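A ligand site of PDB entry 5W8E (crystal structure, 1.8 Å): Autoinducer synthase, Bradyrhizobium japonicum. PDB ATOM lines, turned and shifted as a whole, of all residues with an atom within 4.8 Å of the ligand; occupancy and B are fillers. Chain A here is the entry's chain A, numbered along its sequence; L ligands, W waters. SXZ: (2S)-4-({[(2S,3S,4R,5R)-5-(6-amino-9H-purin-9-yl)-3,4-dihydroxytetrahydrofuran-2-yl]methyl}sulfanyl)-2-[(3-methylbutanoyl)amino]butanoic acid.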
ATOM      1  N   TRP A  36      21.223   0.622  11.860  1.00  0.00           N
ATOM      2  CA  TRP A  36      20.432  -0.046  10.817  1.00  0.00           C
ATOM      3  C   TRP A  36      21.401  -0.913  10.012  1.00  0.00           C
ATOM      4  O   TRP A  36      21.814  -0.550   8.905  1.00  0.00           O
ATOM      5  CB  TRP A  36      19.702   0.951   9.908  1.00  0.00           C
ATOM      6  CG  TRP A  36      18.674   1.811  10.608  1.00  0.00           C
ATOM      7  CD1 TRP A  36      18.315   1.764  11.935  1.00  0.00           C
ATOM      8  CD2 TRP A  36      17.839   2.819  10.014  1.00  0.00           C
ATOM      9  NE1 TRP A  36      17.342   2.699  12.200  1.00  0.00           N
ATOM     10  CE2 TRP A  36      17.028   3.357  11.045  1.00  0.00           C
ATOM     11  CE3 TRP A  36      17.708   3.337   8.714  1.00  0.00           C
ATOM     12  CZ2 TRP A  36      16.093   4.380  10.805  1.00  0.00           C
ATOM     13  CZ3 TRP A  36      16.778   4.352   8.485  1.00  0.00           C
ATOM     14  CH2 TRP A  36      15.990   4.857   9.526  1.00  0.00           C
ATOM     15  N   THR A  38      21.313  -3.604   8.270  1.00  0.00           N
ATOM     16  CA  THR A  38      21.006  -4.088   6.920  1.00  0.00           C
ATOM     17  C   THR A  38      21.532  -3.156   5.828  1.00  0.00           C
ATOM     18  O   THR A  38      21.682  -3.562   4.686  1.00  0.00           O
ATOM     19  CB  THR A  38      19.499  -4.387   6.716  1.00  0.00           C
ATOM     20  OG1 THR A  38      19.333  -5.226   5.580  1.00  0.00           O
ATOM     21  CG2 THR A  38      18.717  -3.101   6.500  1.00  0.00           C
ATOM     22  N   LEU A  39      21.824  -1.904   6.201  1.00  0.00           N
ATOM     23  CA  LEU A  39      22.281  -0.884   5.259  1.00  0.00           C
ATOM     24  C   LEU A  39      23.807  -0.698   5.258  1.00  0.00           C
ATOM     25  O   LEU A  39      24.322   0.116   4.492  1.00  0.00           O
ATOM     26  CB  LEU A  39      21.601   0.456   5.575  1.00  0.00           C
ATOM     27  CG  LEU A  39      20.075   0.505   5.477  1.00  0.00           C
ATOM     28  CD1 LEU A  39      19.579   1.834   6.017  1.00  0.00           C
ATOM     29  CD2 LEU A  39      19.620   0.284   4.038  1.00  0.00           C
ATOM     30  N   ASP A  48      21.059   2.717  -1.241  1.00  0.00           N
ATOM     31  CA  ASP A  48      20.188   1.559  -1.420  1.00  0.00           C
ATOM     32  C   ASP A  48      19.550   1.526  -2.813  1.00  0.00           C
ATOM     33  O   ASP A  48      19.927   2.323  -3.681  1.00  0.00           O
ATOM     34  CB  ASP A  48      19.145   1.451  -0.286  1.00  0.00           C
ATOM     35  CG  ASP A  48      18.049   2.517  -0.365  1.00  0.00           C
ATOM     36  OD1 ASP A  48      17.982   3.271  -1.347  1.00  0.00           O
ATOM     37  OD2 ASP A  48      17.236   2.579   0.593  1.00  0.00           O
ATOM     38  N   TYR A  50      16.886   2.543  -3.901  1.00  0.00           N
ATOM     39  CA  TYR A  50      16.023   3.681  -4.210  1.00  0.00           C
ATOM     40  C   TYR A  50      16.821   4.970  -4.371  1.00  0.00           C
ATOM     41  O   TYR A  50      16.266   6.065  -4.449  1.00  0.00           O
ATOM     42  CB  TYR A  50      14.888   3.779  -3.173  1.00  0.00           C
ATOM     43  CG  TYR A  50      14.301   2.410  -2.910  1.00  0.00           C
ATOM     44  CD1 TYR A  50      13.504   1.788  -3.871  1.00  0.00           C
ATOM     45  CD2 TYR A  50      14.593   1.712  -1.738  1.00  0.00           C
ATOM     46  CE1 TYR A  50      12.992   0.512  -3.658  1.00  0.00           C
ATOM     47  CE2 TYR A  50      14.089   0.442  -1.524  1.00  0.00           C
ATOM     48  CZ  TYR A  50      13.282  -0.150  -2.484  1.00  0.00           C
ATOM     49  OH  TYR A  50      12.785  -1.415  -2.270  1.00  0.00           O
ATOM     50  N   MET A  80      10.461   1.236  -1.307  1.00  0.00           N
ATOM     51  CA  MET A  80      10.692   0.493  -0.072  1.00  0.00           C
ATOM     52  C   MET A  80       9.377   0.019   0.543  1.00  0.00           C
ATOM     53  O   MET A  80       9.270  -1.129   0.972  1.00  0.00           O
ATOM     54  CB  MET A  80      11.499   1.311   0.950  1.00  0.00           C
ATOM     55  CG  MET A  80      11.993   0.476   2.120  1.00  0.00           C
ATOM     56  SD  MET A  80      12.774   1.387   3.445  1.00  0.00           S
ATOM     57  CE  MET A  80      11.374   2.183   4.215  1.00  0.00           C
ATOM     58  N   VAL A  84       9.497  -3.841   0.406  1.00  0.00           N
ATOM     59  CA  VAL A  84      10.014  -4.335   1.675  1.00  0.00           C
ATOM     60  C   VAL A  84       8.940  -4.428   2.767  1.00  0.00           C
ATOM     61  O   VAL A  84       8.895  -5.404   3.520  1.00  0.00           O
ATOM     62  CB  VAL A  84      11.216  -3.501   2.173  1.00  0.00           C
ATOM     63  CG1 VAL A  84      11.870  -4.155   3.394  1.00  0.00           C
ATOM     64  CG2 VAL A  84      12.252  -3.336   1.062  1.00  0.00           C
ATOM     65  N   PHE A  85       8.084  -3.407   2.854  1.00  0.00           N
ATOM     66  CA  PHE A  85       7.097  -3.348   3.940  1.00  0.00           C
ATOM     67  C   PHE A  85       5.624  -3.237   3.497  1.00  0.00           C
ATOM     68  O   PHE A  85       4.867  -2.475   4.102  1.00  0.00           O
ATOM     69  CB  PHE A  85       7.440  -2.179   4.874  1.00  0.00           C
ATOM     70  CG  PHE A  85       8.819  -2.235   5.463  1.00  0.00           C
ATOM     71  CD1 PHE A  85       9.126  -3.148   6.466  1.00  0.00           C
ATOM     72  CD2 PHE A  85       9.809  -1.366   5.015  1.00  0.00           C
ATOM     73  CE1 PHE A  85      10.402  -3.194   7.008  1.00  0.00           C
ATOM     74  CE2 PHE A  85      11.085  -1.411   5.557  1.00  0.00           C
ATOM     75  CZ  PHE A  85      11.378  -2.322   6.558  1.00  0.00           C
ATOM     76  N   TRP A 103       8.808   9.402   1.104  1.00  0.00           N
ATOM     77  CA  TRP A 103       9.697  10.303   1.844  1.00  0.00           C
ATOM     78  C   TRP A 103      10.524   9.453   2.816  1.00  0.00           C
ATOM     79  O   TRP A 103       9.978   8.591   3.498  1.00  0.00           O
ATOM     80  CB  TRP A 103       8.846  11.320   2.614  1.00  0.00           C
ATOM     81  CG  TRP A 103       9.585  12.494   3.206  1.00  0.00           C
ATOM     82  CD1 TRP A 103      10.681  13.131   2.683  1.00  0.00           C
ATOM     83  CD2 TRP A 103       9.240  13.205   4.399  1.00  0.00           C
ATOM     84  NE1 TRP A 103      11.056  14.174   3.493  1.00  0.00           N
ATOM     85  CE2 TRP A 103      10.188  14.246   4.558  1.00  0.00           C
ATOM     86  CE3 TRP A 103       8.231  13.059   5.363  1.00  0.00           C
ATOM     87  CZ2 TRP A 103      10.163  15.130   5.643  1.00  0.00           C
ATOM     88  CZ3 TRP A 103       8.207  13.944   6.448  1.00  0.00           C
ATOM     89  CH2 TRP A 103       9.169  14.970   6.567  1.00  0.00           C
ATOM     90  N   SER A 104      11.833   9.703   2.863  1.00  0.00           N
ATOM     91  CA  SER A 104      12.751   8.832   3.610  1.00  0.00           C
ATOM     92  C   SER A 104      14.084   9.475   3.979  1.00  0.00           C
ATOM     93  O   SER A 104      14.401  10.592   3.543  1.00  0.00           O
ATOM     94  CB  SER A 104      13.004   7.546   2.814  1.00  0.00           C
ATOM     95  OG  SER A 104      13.785   7.807   1.669  1.00  0.00           O
ATOM     96  N   ARG A 105      14.847   8.764   4.813  1.00  0.00           N
ATOM     97  CA  ARG A 105      16.205   9.164   5.232  1.00  0.00           C
ATOM     98  C   ARG A 105      16.306  10.575   5.819  1.00  0.00           C
ATOM     99  O   ARG A 105      17.198  11.347   5.449  1.00  0.00           O
ATOM    100  CB  ARG A 105      17.214   8.948   4.090  1.00  0.00           C
ATOM    101  CG  ARG A 105      17.379   7.498   3.631  1.00  0.00           C
ATOM    102  CD  ARG A 105      17.991   6.601   4.706  1.00  0.00           C
ATOM    103  NE  ARG A 105      18.562   5.403   4.077  1.00  0.00           N
ATOM    104  CZ  ARG A 105      17.866   4.347   3.665  1.00  0.00           C
ATOM    105  NH1 ARG A 105      16.556   4.285   3.828  1.00  0.00           N
ATOM    106  NH2 ARG A 105      18.505   3.336   3.080  1.00  0.00           N
ATOM    107  N   TYR A 106      15.405  10.896   6.743  1.00  0.00           N
ATOM    108  CA  TYR A 106      15.404  12.194   7.427  1.00  0.00           C
ATOM    109  C   TYR A 106      16.543  12.198   8.433  1.00  0.00           C
ATOM    110  O   TYR A 106      16.606  11.329   9.310  1.00  0.00           O
ATOM    111  CB  TYR A 106      14.066  12.376   8.142  1.00  0.00           C
ATOM    112  CG  TYR A 106      13.754  13.779   8.669  1.00  0.00           C
ATOM    113  CD1 TYR A 106      14.434  14.302   9.767  1.00  0.00           C
ATOM    114  CD2 TYR A 106      12.738  14.540   8.090  1.00  0.00           C
ATOM    115  CE1 TYR A 106      14.126  15.571  10.267  1.00  0.00           C
ATOM    116  CE2 TYR A 106      12.414  15.797   8.578  1.00  0.00           C
ATOM    117  CZ  TYR A 106      13.107  16.305   9.667  1.00  0.00           C
ATOM    118  OH  TYR A 106      12.776  17.557  10.135  1.00  0.00           O
ATOM    119  N   ALA A 139       5.348   7.385   3.827  1.00  0.00           N
ATOM    120  CA  ALA A 139       6.543   7.030   4.580  1.00  0.00           C
ATOM    121  C   ALA A 139       6.357   5.738   5.357  1.00  0.00           C
ATOM    122  O   ALA A 139       5.272   5.446   5.827  1.00  0.00           O
ATOM    123  CB  ALA A 139       6.935   8.149   5.525  1.00  0.00           C
ATOM    124  N   ILE A 140       7.445   4.978   5.490  1.00  0.00           N
ATOM    125  CA  ILE A 140       7.589   4.007   6.558  1.00  0.00           C
ATOM    126  C   ILE A 140       8.344   4.749   7.652  1.00  0.00           C
ATOM    127  O   ILE A 140       9.425   5.300   7.395  1.00  0.00           O
ATOM    128  CB  ILE A 140       8.386   2.765   6.094  1.00  0.00           C
ATOM    129  CG1 ILE A 140       7.623   1.981   5.007  1.00  0.00           C
ATOM    130  CG2 ILE A 140       8.796   1.906   7.287  1.00  0.00           C
ATOM    131  CD1 ILE A 140       6.283   1.399   5.434  1.00  0.00           C
ATOM    132  N   MET A 141       7.784   4.788   8.858  1.00  0.00           N
ATOM    133  CA  MET A 141       8.370   5.577   9.932  1.00  0.00           C
ATOM    134  C   MET A 141       8.236   4.951  11.307  1.00  0.00           C
ATOM    135  O   MET A 141       7.265   4.231  11.584  1.00  0.00           O
ATOM    136  CB  MET A 141       7.731   6.971   9.963  1.00  0.00           C
ATOM    137  CG  MET A 141       6.283   6.970  10.410  1.00  0.00           C
ATOM    138  SD  MET A 141       5.460   8.474   9.880  1.00  0.00           S
ATOM    139  CE  MET A 141       4.127   8.512  11.071  1.00  0.00           C
ATOM    140  N   GLU A 142       9.196   5.233  12.174  1.00  0.00           N
ATOM    141  CA  GLU A 142       9.101   4.871  13.575  1.00  0.00           C
ATOM    142  C   GLU A 142       7.906   5.619  14.166  1.00  0.00           C
ATOM    143  O   GLU A 142       7.644   6.767  13.781  1.00  0.00           O
ATOM    144  CB  GLU A 142      10.385   5.256  14.319  1.00  0.00           C
ATOM    145  CG  GLU A 142      11.670   4.712  13.693  1.00  0.00           C
ATOM    146  CD  GLU A 142      12.335   5.661  12.703  1.00  0.00           C
ATOM    147  OE1 GLU A 142      11.637   6.359  11.933  1.00  0.00           O
ATOM    148  OE2 GLU A 142      13.583   5.716  12.695  1.00  0.00           O
ATOM    149  N   TRP A 145       7.486   9.349  15.309  1.00  0.00           N
ATOM    150  CA  TRP A 145       7.274  10.432  14.342  1.00  0.00           C
ATOM    151  C   TRP A 145       5.894  11.089  14.484  1.00  0.00           C
ATOM    152  O   TRP A 145       5.727  12.259  14.127  1.00  0.00           O
ATOM    153  CB  TRP A 145       7.503   9.945  12.910  1.00  0.00           C
ATOM    154  CG  TRP A 145       8.923  10.101  12.468  1.00  0.00           C
ATOM    155  CD1 TRP A 145       9.872   9.111  12.349  1.00  0.00           C
ATOM    156  CD2 TRP A 145       9.574  11.317  12.082  1.00  0.00           C
ATOM    157  NE1 TRP A 145      11.062   9.643  11.908  1.00  0.00           N
ATOM    158  CE2 TRP A 145      10.910  10.999  11.742  1.00  0.00           C
ATOM    159  CE3 TRP A 145       9.163  12.655  12.006  1.00  0.00           C
ATOM    160  CZ2 TRP A 145      11.835  11.970  11.323  1.00  0.00           C
ATOM    161  CZ3 TRP A 145      10.072  13.614  11.586  1.00  0.00           C
ATOM    162  CH2 TRP A 145      11.395  13.262  11.253  1.00  0.00           C
ATOM    163  N   PHE A 149       5.182  14.977  13.666  1.00  0.00           N
ATOM    164  CA  PHE A 149       4.311  15.383  12.569  1.00  0.00           C
ATOM    165  C   PHE A 149       3.216  16.329  13.077  1.00  0.00           C
ATOM    166  O   PHE A 149       2.959  17.368  12.476  1.00  0.00           O
ATOM    167  CB  PHE A 149       3.654  14.157  11.920  1.00  0.00           C
ATOM    168  CG  PHE A 149       4.541  13.427  10.935  1.00  0.00           C
ATOM    169  CD1 PHE A 149       5.879  13.772  10.758  1.00  0.00           C
ATOM    170  CD2 PHE A 149       4.035  12.363  10.205  1.00  0.00           C
ATOM    171  CE1 PHE A 149       6.680  13.079   9.859  1.00  0.00           C
ATOM    172  CE2 PHE A 149       4.829  11.663   9.295  1.00  0.00           C
ATOM    173  CZ  PHE A 149       6.154  12.024   9.128  1.00  0.00           C
ATOM    174  N   VAL A 165       9.526  -3.682  13.606  1.00  0.00           N
ATOM    175  CA  VAL A 165      10.524  -3.881  12.564  1.00  0.00           C
ATOM    176  C   VAL A 165      11.876  -3.782  13.269  1.00  0.00           C
ATOM    177  O   VAL A 165      12.237  -2.727  13.778  1.00  0.00           O
ATOM    178  CB  VAL A 165      10.419  -2.832  11.423  1.00  0.00           C
ATOM    179  CG1 VAL A 165      11.598  -2.934  10.469  1.00  0.00           C
ATOM    180  CG2 VAL A 165       9.111  -2.998  10.658  1.00  0.00           C
ATOM    181  N   GLU A 166      12.587  -4.898  13.317  1.00  0.00           N
ATOM    182  CA  GLU A 166      13.877  -4.983  13.999  1.00  0.00           C
ATOM    183  C   GLU A 166      13.860  -4.302  15.376  1.00  0.00           C
ATOM    184  O   GLU A 166      14.648  -3.379  15.628  1.00  0.00           O
ATOM    185  CB  GLU A 166      15.000  -4.428  13.103  1.00  0.00           C
ATOM    186  CG  GLU A 166      16.377  -5.010  13.386  1.00  0.00           C
ATOM    187  CD  GLU A 166      16.388  -6.534  13.354  1.00  0.00           C
ATOM    188  OE1 GLU A 166      16.107  -7.111  12.282  1.00  0.00           O
ATOM    189  OE2 GLU A 166      16.688  -7.140  14.400  1.00  0.00           O
ATOM    190  N   THR A 170       6.972   0.492  14.204  1.00  0.00           N
ATOM    191  CA  THR A 170       7.069   1.141  12.897  1.00  0.00           C
ATOM    192  C   THR A 170       5.692   1.136  12.245  1.00  0.00           C
ATOM    193  O   THR A 170       4.884   0.264  12.526  1.00  0.00           O
ATOM    194  CB  THR A 170       8.079   0.366  12.009  1.00  0.00           C
ATOM    195  OG1 THR A 170       9.320   0.258  12.716  1.00  0.00           O
ATOM    196  CG2 THR A 170       8.327   1.066  10.686  1.00  0.00           C
HETATM  197  OXT SXZ L   1      12.573   5.318   4.764  1.00  0.00           O
HETATM  198  C   SXZ L   1      13.477   5.633   5.577  1.00  0.00           C
HETATM  199  O   SXZ L   1      14.636   5.894   5.212  1.00  0.00           O
HETATM  200  CA  SXZ L   1      13.130   5.683   7.050  1.00  0.00           C
HETATM  201  N   SXZ L   1      11.989   6.556   7.320  1.00  0.00           N
HETATM  202  CB  SXZ L   1      12.753   4.272   7.507  1.00  0.00           C
HETATM  203  CG  SXZ L   1      12.228   4.165   8.939  1.00  0.00           C
HETATM  204  SD  SXZ L   1      12.102   2.467   9.400  1.00  0.00           S
HETATM  205  C5' SXZ L   1      13.726   1.919   9.823  1.00  0.00           C
HETATM  206  C4' SXZ L   1      13.984   0.501   9.322  1.00  0.00           C
HETATM  207  O4' SXZ L   1      13.937   0.470   7.892  1.00  0.00           O
HETATM  208  C1' SXZ L   1      15.008  -0.344   7.398  1.00  0.00           C
HETATM  209  C2' SXZ L   1      16.131  -0.152   8.412  1.00  0.00           C
HETATM  210  O2' SXZ L   1      17.007  -1.270   8.452  1.00  0.00           O
HETATM  211  C3' SXZ L   1      15.368   0.011   9.720  1.00  0.00           C
HETATM  212  O3' SXZ L   1      15.251  -1.255  10.373  1.00  0.00           O
HETATM  213  N9  SXZ L   1      15.373   0.056   6.018  1.00  0.00           N
HETATM  214  C8  SXZ L   1      15.673   1.298   5.578  1.00  0.00           C
HETATM  215  N7  SXZ L   1      15.951   1.235   4.250  1.00  0.00           N
HETATM  216  C5  SXZ L   1      15.806  -0.046   3.867  1.00  0.00           C
HETATM  217  C6  SXZ L   1      15.950  -0.718   2.650  1.00  0.00           C
HETATM  218  N6  SXZ L   1      16.302  -0.052   1.523  1.00  0.00           N
HETATM  219  N1  SXZ L   1      15.724  -2.057   2.600  1.00  0.00           N
HETATM  220  C2  SXZ L   1      15.378  -2.743   3.696  1.00  0.00           C
HETATM  221  N3  SXZ L   1      15.237  -2.119   4.870  1.00  0.00           N
HETATM  222  C4  SXZ L   1      15.444  -0.781   4.980  1.00  0.00           C
HETATM  223  C1  SXZ L   1      12.100   7.861   7.622  1.00  0.00           C
HETATM  224  O2  SXZ L   1      13.171   8.445   7.697  1.00  0.00           O
HETATM  225  C3  SXZ L   1      10.785   8.580   7.902  1.00  0.00           C
HETATM  226  C7  SXZ L   1      10.879  10.107   7.872  1.00  0.00           C
HETATM  227  C9  SXZ L   1       9.582  10.716   8.390  1.00  0.00           C
HETATM  228  C10 SXZ L   1      11.157  10.629   6.462  1.00  0.00           C
HETATM  229  O   HOH W   1      17.434  -1.493  -1.013  1.00  0.00           O
HETATM  230  O   HOH W   2      14.670  -4.198   6.827  1.00  0.00           O
HETATM  231  O   HOH W   3       9.975   5.901   4.081  1.00  0.00           O
HETATM  232  O   HOH W   4      17.511  -1.868  12.766  1.00  0.00           O
HETATM  233  O   HOH W   5      11.725   1.371  12.553  1.00  0.00           O
HETATM  234  O   HOH W   6      13.827  -0.818  12.670  1.00  0.00           O
HETATM  235  O   HOH W   7      15.904  -3.977   0.603  1.00  0.00           O
HETATM  236  O   HOH W   8      13.639   7.912  10.617  1.00  0.00           O
HETATM  237  O   HOH W   9      13.339   4.316   2.141  1.00  0.00           O
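O of Ile 140 is in hydrogen-bond range of N of the ligand, 2.9 Å away. N of Tyr 106 lies within hydrogen-bond range of O2 of the ligand, at 3.5 Å. The side-chain carboxylate of Asp 48 is in hydrogen-bond range of a nitrogen (N6) of the ligand, 2.9 Å away. The backbone NH (N) of Arg 105 is in hydrogen-bond range of an oxygen (O) of the ligand (2.9 Å). The guanidinium group of Arg 105 is in salt-bridge range of an oxygen (O) of the ligand (2.9 Å).
The side-chain carboxylate (OD1) of Asp 48 sits at hydrogen-bond distance from the backbone NH (N) of Tyr 50 (2.9 Å). The indole nitrogen (NE1) of Trp 145 sits close to the side-chain carboxylate (OE1) of Glu 142 (3.3 Å). The guanidinium group of Arg 105 is in salt-bridge range of the side-chain carboxylate of Asp 48. O of Met 80 lies within hydrogen-bond range of N of Phe 85, 3.2 Å away.
SD of Met 80 lies close to N7 of the ligand. Trp 36 touches the ligand (CZ2 to C5', 3.6 Å). Thr 38 touches the ligand. CD2 of Leu 39 touches N7 of the ligand, 3.8 Å away. Tyr 50 touches the ligand (CE2 to N6, 3.8 Å). Val 84 touches the ligand. Trp 103 touches the ligand (O to C10, 3.8 Å). Ser 104 touches the ligand. Glu 142 touches the ligand. Trp 145 touches the ligand (CE2 to C9, 3.6 Å). CZ of Phe 149 touches C9 of the ligand, 3.7 Å away. Hydrophobic or aromatic side chains that line the ligand: Trp 36, Leu 39, Tyr 50, Met 80, Val 84, Trp 103, Tyr 106, Ile 140, Trp 145 and Phe 149. Within 4 Å of the ligand: Trp 36, Thr 38, Leu 39, Asp 48, Tyr 50, Met 80, Val 84, Trp 103, Ser 104, Arg 105, Tyr 106, Ile 140, Glu 142, Trp 145 and Phe 149.
Water W6 bridges O of Val 165 (2.7 Å) and O3' of the ligand (2.7 Å). Water W3 lies within hydrogen-bond range of OXT of the ligand, O of Trp 103 and N of Ile 140. Water W9 lies within hydrogen-bond range of OXT of the ligand and SD of Met 80. Water W8 lies within hydrogen-bond range of OE1 of Glu 142, O2 of the ligand and NE1 of Trp 145. Water W5 lies within hydrogen-bond range of OG1 of Thr 170 (2.7 Å) and SD of the ligand (3.4 Å).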
